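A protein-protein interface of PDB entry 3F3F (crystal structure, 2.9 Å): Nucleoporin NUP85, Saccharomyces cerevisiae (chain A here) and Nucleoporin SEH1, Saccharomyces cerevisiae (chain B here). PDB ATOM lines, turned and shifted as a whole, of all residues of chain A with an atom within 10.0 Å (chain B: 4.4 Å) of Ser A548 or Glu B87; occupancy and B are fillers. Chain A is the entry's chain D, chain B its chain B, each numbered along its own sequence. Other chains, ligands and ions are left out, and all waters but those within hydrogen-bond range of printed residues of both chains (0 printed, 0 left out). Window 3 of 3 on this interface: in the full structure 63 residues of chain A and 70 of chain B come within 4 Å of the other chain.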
ATOM      1  N   THR A 541      -3.628 -13.172 -15.704  1.00  0.00           N
ATOM      2  CA  THR A 541      -4.623 -12.227 -16.185  1.00  0.00           C
ATOM      3  C   THR A 541      -5.253 -11.573 -14.970  1.00  0.00           C
ATOM      4  O   THR A 541      -5.335 -10.340 -14.870  1.00  0.00           O
ATOM      5  CB  THR A 541      -5.718 -12.950 -16.966  1.00  0.00           C
ATOM      6  OG1 THR A 541      -5.148 -13.552 -18.130  1.00  0.00           O
ATOM      7  CG2 THR A 541      -6.806 -11.980 -17.376  1.00  0.00           C
ATOM      8  N   LEU A 542      -5.691 -12.440 -14.059  1.00  0.00           N
ATOM      9  CA  LEU A 542      -6.326 -12.083 -12.792  1.00  0.00           C
ATOM     10  C   LEU A 542      -5.613 -10.943 -12.057  1.00  0.00           C
ATOM     11  O   LEU A 542      -6.252 -10.045 -11.497  1.00  0.00           O
ATOM     12  CB  LEU A 542      -6.359 -13.314 -11.864  1.00  0.00           C
ATOM     13  CG  LEU A 542      -7.687 -13.521 -11.127  1.00  0.00           C
ATOM     14  CD1 LEU A 542      -8.634 -14.148 -12.127  1.00  0.00           C
ATOM     15  CD2 LEU A 542      -7.594 -14.345  -9.849  1.00  0.00           C
ATOM     16  N   GLY A 543      -4.283 -10.995 -12.063  1.00  0.00           N
ATOM     17  CA  GLY A 543      -3.499  -9.997 -11.359  1.00  0.00           C
ATOM     18  C   GLY A 543      -2.654  -8.982 -12.116  1.00  0.00           C
ATOM     19  O   GLY A 543      -1.793  -8.351 -11.496  1.00  0.00           O
ATOM     20  N   ASN A 544      -2.862  -8.815 -13.425  1.00  0.00           N
ATOM     21  CA  ASN A 544      -2.087  -7.820 -14.180  1.00  0.00           C
ATOM     22  C   ASN A 544      -2.563  -6.485 -13.624  1.00  0.00           C
ATOM     23  O   ASN A 544      -1.844  -5.482 -13.638  1.00  0.00           O
ATOM     24  CB  ASN A 544      -2.400  -7.883 -15.681  1.00  0.00           C
ATOM     25  CG  ASN A 544      -1.147  -7.824 -16.538  1.00  0.00           C
ATOM     26  OD1 ASN A 544      -0.543  -8.848 -16.853  1.00  0.00           O
ATOM     27  ND2 ASN A 544      -0.742  -6.619 -16.903  1.00  0.00           N
ATOM     28  N   GLN A 545      -3.795  -6.517 -13.124  1.00  0.00           N
ATOM     29  CA  GLN A 545      -4.464  -5.373 -12.526  1.00  0.00           C
ATOM     30  C   GLN A 545      -3.596  -4.764 -11.421  1.00  0.00           C
ATOM     31  O   GLN A 545      -3.782  -3.606 -11.042  1.00  0.00           O
ATOM     32  CB  GLN A 545      -5.823  -5.824 -11.958  1.00  0.00           C
ATOM     33  CG  GLN A 545      -6.631  -6.734 -12.915  1.00  0.00           C
ATOM     34  CD  GLN A 545      -8.097  -6.931 -12.503  1.00  0.00           C
ATOM     35  OE1 GLN A 545      -8.888  -5.984 -12.501  1.00  0.00           O
ATOM     36  NE2 GLN A 545      -8.462  -8.167 -12.163  1.00  0.00           N
ATOM     37  N   MET A 546      -2.642  -5.552 -10.922  1.00  0.00           N
ATOM     38  CA  MET A 546      -1.738  -5.112  -9.859  1.00  0.00           C
ATOM     39  C   MET A 546      -0.631  -4.189 -10.352  1.00  0.00           C
ATOM     40  O   MET A 546      -0.187  -3.298  -9.625  1.00  0.00           O
ATOM     41  CB  MET A 546      -1.095  -6.318  -9.161  1.00  0.00           C
ATOM     42  CG  MET A 546      -2.068  -7.234  -8.438  1.00  0.00           C
ATOM     43  SD  MET A 546      -1.276  -8.328  -7.235  1.00  0.00           S
ATOM     44  CE  MET A 546      -2.036  -7.786  -5.634  1.00  0.00           C
ATOM     45  N   LEU A 547      -0.190  -4.397 -11.588  1.00  0.00           N
ATOM     46  CA  LEU A 547       0.886  -3.594 -12.159  1.00  0.00           C
ATOM     47  C   LEU A 547       0.447  -2.235 -12.723  1.00  0.00           C
ATOM     48  O   LEU A 547       1.281  -1.486 -13.235  1.00  0.00           O
ATOM     49  CB  LEU A 547       1.593  -4.404 -13.244  1.00  0.00           C
ATOM     50  CG  LEU A 547       1.674  -5.899 -12.934  1.00  0.00           C
ATOM     51  CD1 LEU A 547       2.415  -6.606 -14.046  1.00  0.00           C
ATOM     52  CD2 LEU A 547       2.358  -6.110 -11.599  1.00  0.00           C
ATOM     53  N   SER A 548      -0.849  -1.922 -12.633  1.00  0.00           N
ATOM     54  CA  SER A 548      -1.385  -0.640 -13.128  1.00  0.00           C
ATOM     55  C   SER A 548      -2.078   0.177 -12.014  1.00  0.00           C
ATOM     56  O   SER A 548      -2.663   1.241 -12.276  1.00  0.00           O
ATOM     57  CB  SER A 548      -2.370  -0.866 -14.297  1.00  0.00           C
ATOM     58  OG  SER A 548      -3.612  -1.409 -13.869  1.00  0.00           O
ATOM     59  N   ALA A 549      -1.999  -0.329 -10.781  1.00  0.00           N
ATOM     60  CA  ALA A 549      -2.594   0.330  -9.622  1.00  0.00           C
ATOM     61  C   ALA A 549      -1.497   0.872  -8.701  1.00  0.00           C
ATOM     62  O   ALA A 549      -0.311   0.571  -8.943  1.00  0.00           O
ATOM     63  CB  ALA A 549      -3.493  -0.657  -8.857  1.00  0.00           C
ATOM     64  N   ARG B  72      -4.844  -4.030 -19.688  1.00  0.00           N
ATOM     65  CA  ARG B  72      -5.917  -3.445 -20.485  1.00  0.00           C
ATOM     66  C   ARG B  72      -5.253  -2.557 -21.515  1.00  0.00           C
ATOM     67  O   ARG B  72      -4.928  -1.420 -21.227  1.00  0.00           O
ATOM     68  CB  ARG B  72      -6.828  -2.628 -19.575  1.00  0.00           C
ATOM     69  CG  ARG B  72      -7.572  -3.481 -18.571  1.00  0.00           C
ATOM     70  CD  ARG B  72      -8.757  -4.171 -19.232  1.00  0.00           C
ATOM     71  NE  ARG B  72      -9.896  -3.258 -19.366  1.00  0.00           N
ATOM     72  CZ  ARG B  72     -11.003  -3.513 -20.063  1.00  0.00           C
ATOM     73  NH1 ARG B  72     -11.144  -4.665 -20.710  1.00  0.00           N
ATOM     74  NH2 ARG B  72     -11.978  -2.613 -20.098  1.00  0.00           N
ATOM     75  N   TRP B  86      -2.568   2.330 -25.894  1.00  0.00           N
ATOM     76  CA  TRP B  86      -3.100   2.922 -24.679  1.00  0.00           C
ATOM     77  C   TRP B  86      -3.331   1.878 -23.610  1.00  0.00           C
ATOM     78  O   TRP B  86      -3.606   0.726 -23.926  1.00  0.00           O
ATOM     79  CB  TRP B  86      -4.418   3.620 -24.987  1.00  0.00           C
ATOM     80  CG  TRP B  86      -4.414   4.286 -26.308  1.00  0.00           C
ATOM     81  CD1 TRP B  86      -4.472   3.681 -27.530  1.00  0.00           C
ATOM     82  CD2 TRP B  86      -4.302   5.687 -26.560  1.00  0.00           C
ATOM     83  NE1 TRP B  86      -4.404   4.620 -28.534  1.00  0.00           N
ATOM     84  CE2 TRP B  86      -4.297   5.861 -27.965  1.00  0.00           C
ATOM     85  CE3 TRP B  86      -4.199   6.815 -25.734  1.00  0.00           C
ATOM     86  CZ2 TRP B  86      -4.195   7.121 -28.564  1.00  0.00           C
ATOM     87  CZ3 TRP B  86      -4.098   8.071 -26.332  1.00  0.00           C
ATOM     88  CH2 TRP B  86      -4.095   8.211 -27.736  1.00  0.00           C
ATOM     89  N   GLU B  87      -3.216   2.286 -22.349  1.00  0.00           N
ATOM     90  CA  GLU B  87      -3.447   1.388 -21.226  1.00  0.00           C
ATOM     91  C   GLU B  87      -4.421   2.036 -20.262  1.00  0.00           C
ATOM     92  O   GLU B  87      -4.245   3.179 -19.863  1.00  0.00           O
ATOM     93  CB  GLU B  87      -2.152   1.061 -20.494  1.00  0.00           C
ATOM     94  CG  GLU B  87      -2.368   0.245 -19.232  1.00  0.00           C
ATOM     95  CD  GLU B  87      -1.071  -0.318 -18.668  1.00  0.00           C
ATOM     96  OE1 GLU B  87      -1.096  -0.868 -17.541  1.00  0.00           O
ATOM     97  OE2 GLU B  87      -0.026  -0.216 -19.351  1.00  0.00           O
ATOM     98  N   GLU B  88      -5.454   1.298 -19.887  1.00  0.00           N
ATOM     99  CA  GLU B  88      -6.459   1.826 -18.985  1.00  0.00           C
ATOM    100  C   GLU B  88      -5.938   1.992 -17.572  1.00  0.00           C
ATOM    101  O   GLU B  88      -5.313   1.088 -17.010  1.00  0.00           O
ATOM    102  CB  GLU B  88      -7.693   0.917 -18.972  1.00  0.00           C
ATOM    103  CG  GLU B  88      -8.852   1.469 -18.141  1.00  0.00           C
ATOM    104  CD  GLU B  88     -10.139   0.681 -18.312  1.00  0.00           C
ATOM    105  OE1 GLU B  88     -10.154  -0.518 -17.939  1.00  0.00           O
ATOM    106  OE2 GLU B  88     -11.127   1.270 -18.821  1.00  0.00           O
ATOM    107  N   ASP B  89      -6.200   3.170 -17.014  1.00  0.00           N
ATOM    108  CA  ASP B  89      -5.803   3.492 -15.649  1.00  0.00           C
ATOM    109  C   ASP B  89      -7.082   3.441 -14.823  1.00  0.00           C
ATOM    110  O   ASP B  89      -7.843   4.403 -14.787  1.00  0.00           O
ATOM    111  CB  ASP B  89      -5.167   4.895 -15.585  1.00  0.00           C
ATOM    112  CG  ASP B  89      -4.908   5.363 -14.157  1.00  0.00           C
ATOM    113  OD1 ASP B  89      -4.436   4.539 -13.335  1.00  0.00           O
ATOM    114  OD2 ASP B  89      -5.167   6.556 -13.868  1.00  0.00           O
ATOM    115  N   PRO B  90      -7.332   2.309 -14.149  1.00  0.00           N
ATOM    116  CA  PRO B  90      -8.522   2.094 -13.314  1.00  0.00           C
ATOM    117  C   PRO B  90      -8.761   3.146 -12.240  1.00  0.00           C
ATOM    118  O   PRO B  90      -9.832   3.189 -11.638  1.00  0.00           O
ATOM    119  CB  PRO B  90      -8.275   0.715 -12.712  1.00  0.00           C
ATOM    120  CG  PRO B  90      -6.783   0.670 -12.612  1.00  0.00           C
ATOM    121  CD  PRO B  90      -6.358   1.223 -13.950  1.00  0.00           C
ATOM    122  N   ASP B  91      -7.762   3.993 -12.010  1.00  0.00           N
ATOM    123  CA  ASP B  91      -7.842   5.041 -10.994  1.00  0.00           C
ATOM    124  C   ASP B  91      -8.316   6.382 -11.551  1.00  0.00           C
ATOM    125  O   ASP B  91      -7.892   7.441 -11.084  1.00  0.00           O
ATOM    126  CB  ASP B  91      -6.473   5.214 -10.334  1.00  0.00           C
ATOM    127  CG  ASP B  91      -5.938   3.913  -9.765  1.00  0.00           C
ATOM    128  OD1 ASP B  91      -6.562   3.389  -8.818  1.00  0.00           O
ATOM    129  OD2 ASP B  91      -4.904   3.412 -10.269  1.00  0.00           O
ATOM    130  N   ARG B  99      -9.117   8.289 -19.053  1.00  0.00           N
ATOM    131  CA  ARG B  99      -9.085   6.934 -18.518  1.00  0.00           C
ATOM    132  C   ARG B  99      -8.083   6.032 -19.219  1.00  0.00           C
ATOM    133  O   ARG B  99      -7.700   4.985 -18.690  1.00  0.00           O
ATOM    134  CB  ARG B  99     -10.492   6.327 -18.547  1.00  0.00           C
ATOM    135  CG  ARG B  99     -10.638   5.086 -17.700  1.00  0.00           C
ATOM    136  CD  ARG B  99     -12.090   4.824 -17.367  1.00  0.00           C
ATOM    137  NE  ARG B  99     -12.289   3.507 -16.767  1.00  0.00           N
ATOM    138  CZ  ARG B  99     -11.731   3.104 -15.629  1.00  0.00           C
ATOM    139  NH1 ARG B  99     -10.935   3.922 -14.961  1.00  0.00           N
ATOM    140  NH2 ARG B  99     -11.957   1.881 -15.162  1.00  0.00           N
ATOM    141  N   TRP B 100      -7.645   6.455 -20.403  1.00  0.00           N
ATOM    142  CA  TRP B 100      -6.670   5.689 -21.176  1.00  0.00           C
ATOM    143  C   TRP B 100      -5.423   6.525 -21.515  1.00  0.00           C
ATOM    144  O   TRP B 100      -5.508   7.507 -22.265  1.00  0.00           O
ATOM    145  CB  TRP B 100      -7.325   5.158 -22.459  1.00  0.00           C
ATOM    146  CG  TRP B 100      -8.363   4.090 -22.205  1.00  0.00           C
ATOM    147  CD1 TRP B 100      -9.628   4.265 -21.714  1.00  0.00           C
ATOM    148  CD2 TRP B 100      -8.206   2.683 -22.400  1.00  0.00           C
ATOM    149  NE1 TRP B 100     -10.264   3.055 -21.590  1.00  0.00           N
ATOM    150  CE2 TRP B 100      -9.411   2.067 -22.005  1.00  0.00           C
ATOM    151  CE3 TRP B 100      -7.158   1.882 -22.872  1.00  0.00           C
ATOM    152  CZ2 TRP B 100      -9.599   0.687 -22.068  1.00  0.00           C
ATOM    153  CZ3 TRP B 100      -7.344   0.509 -22.935  1.00  0.00           C
ATOM    154  CH2 TRP B 100      -8.556  -0.074 -22.534  1.00  0.00           C
ATOM    155  N   ASN B 101      -4.273   6.124 -20.959  1.00  0.00           N
ATOM    156  CA  ASN B 101      -3.000   6.819 -21.164  1.00  0.00           C
ATOM    157  C   ASN B 101      -2.204   6.303 -22.340  1.00  0.00           C
ATOM    158  O   ASN B 101      -1.950   5.104 -22.436  1.00  0.00           O
ATOM    159  CB  ASN B 101      -2.094   6.683 -19.942  1.00  0.00           C
ATOM    160  CG  ASN B 101      -2.782   7.070 -18.657  1.00  0.00           C
ATOM    161  OD1 ASN B 101      -3.523   6.283 -18.071  1.00  0.00           O
ATOM    162  ND2 ASN B 101      -2.546   8.295 -18.208  1.00  0.00           N
ATOM    163  N   LEU B 103       0.665   5.001 -24.309  1.00  0.00           N
ATOM    164  CA  LEU B 103       1.858   4.314 -23.859  1.00  0.00           C
ATOM    165  C   LEU B 103       2.984   4.493 -24.850  1.00  0.00           C
ATOM    166  O   LEU B 103       4.149   4.221 -24.537  1.00  0.00           O
ATOM    167  CB  LEU B 103       1.589   2.818 -23.715  1.00  0.00           C
ATOM    168  CG  LEU B 103       0.666   2.340 -22.603  1.00  0.00           C
ATOM    169  CD1 LEU B 103       0.590   0.815 -22.647  1.00  0.00           C
ATOM    170  CD2 LEU B 103       1.194   2.827 -21.255  1.00  0.00           C
ATOM    171  N   LEU B 147       5.571  -1.287 -21.080  1.00  0.00           N
ATOM    172  CA  LEU B 147       4.612  -1.199 -22.159  1.00  0.00           C
ATOM    173  C   LEU B 147       4.823   0.097 -22.948  1.00  0.00           C
ATOM    174  O   LEU B 147       3.866   0.743 -23.370  1.00  0.00           O
ATOM    175  CB  LEU B 147       3.192  -1.287 -21.591  1.00  0.00           C
ATOM    176  CG  LEU B 147       2.936  -2.541 -20.736  1.00  0.00           C
ATOM    177  CD1 LEU B 147       1.495  -2.555 -20.262  1.00  0.00           C
ATOM    178  CD2 LEU B 147       3.234  -3.801 -21.540  1.00  0.00           C
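Of the 12 printed residues of chain B, 4 touch a printed residue of chain A. Hydrophobic or aromatic side chains of chain B that line the printed part of chain A: Pro B90. Among the printed residues, no Asp or Glu carboxylate lies within 4 Å of a Lys or Arg side-chain nitrogen of the other chain.
Ser A548 touches just these residues of chain B: Glu B87, Asp B89, Pro B90 and Asp B91. Of chain A, only Ser A548 (3.5 Å) comes within 4 Å of Glu B87. No residue of chain A comes within 4 Å of Asn B101. Of the printed residues of chain A, Asp B89 touches Ser A548 (3.9 Å). Printed residues of chain A within 4 Å of Asp B91: Ser A548 and Ala A549. Leu A542 touches none of the printed residues of chain B. The nearest printed residue of chain A that does not touch Asp B91 is Gln A545 (7.1 Å).
The backbone carbonyl oxygen (O) of Asn B101 lies within hydrogen-bond range of the backbone NH (N) of Glu B87. The backbone NH of Asp B89 lies within hydrogen-bond range of the backbone carbonyl oxygen of Arg B99.
Glu B87 touches Ser A548 (OE1 to CB, 3.5 Å). Asp B89 touches Ser A548 (OD1 to O, 3.9 Å). CD of Pro B90 touches OG of Ser A548, at 3.8 Å. O of Ser A548 touches OD2 of Asp B91, at 3.7 Å. Ala A549 touches Asp B91.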
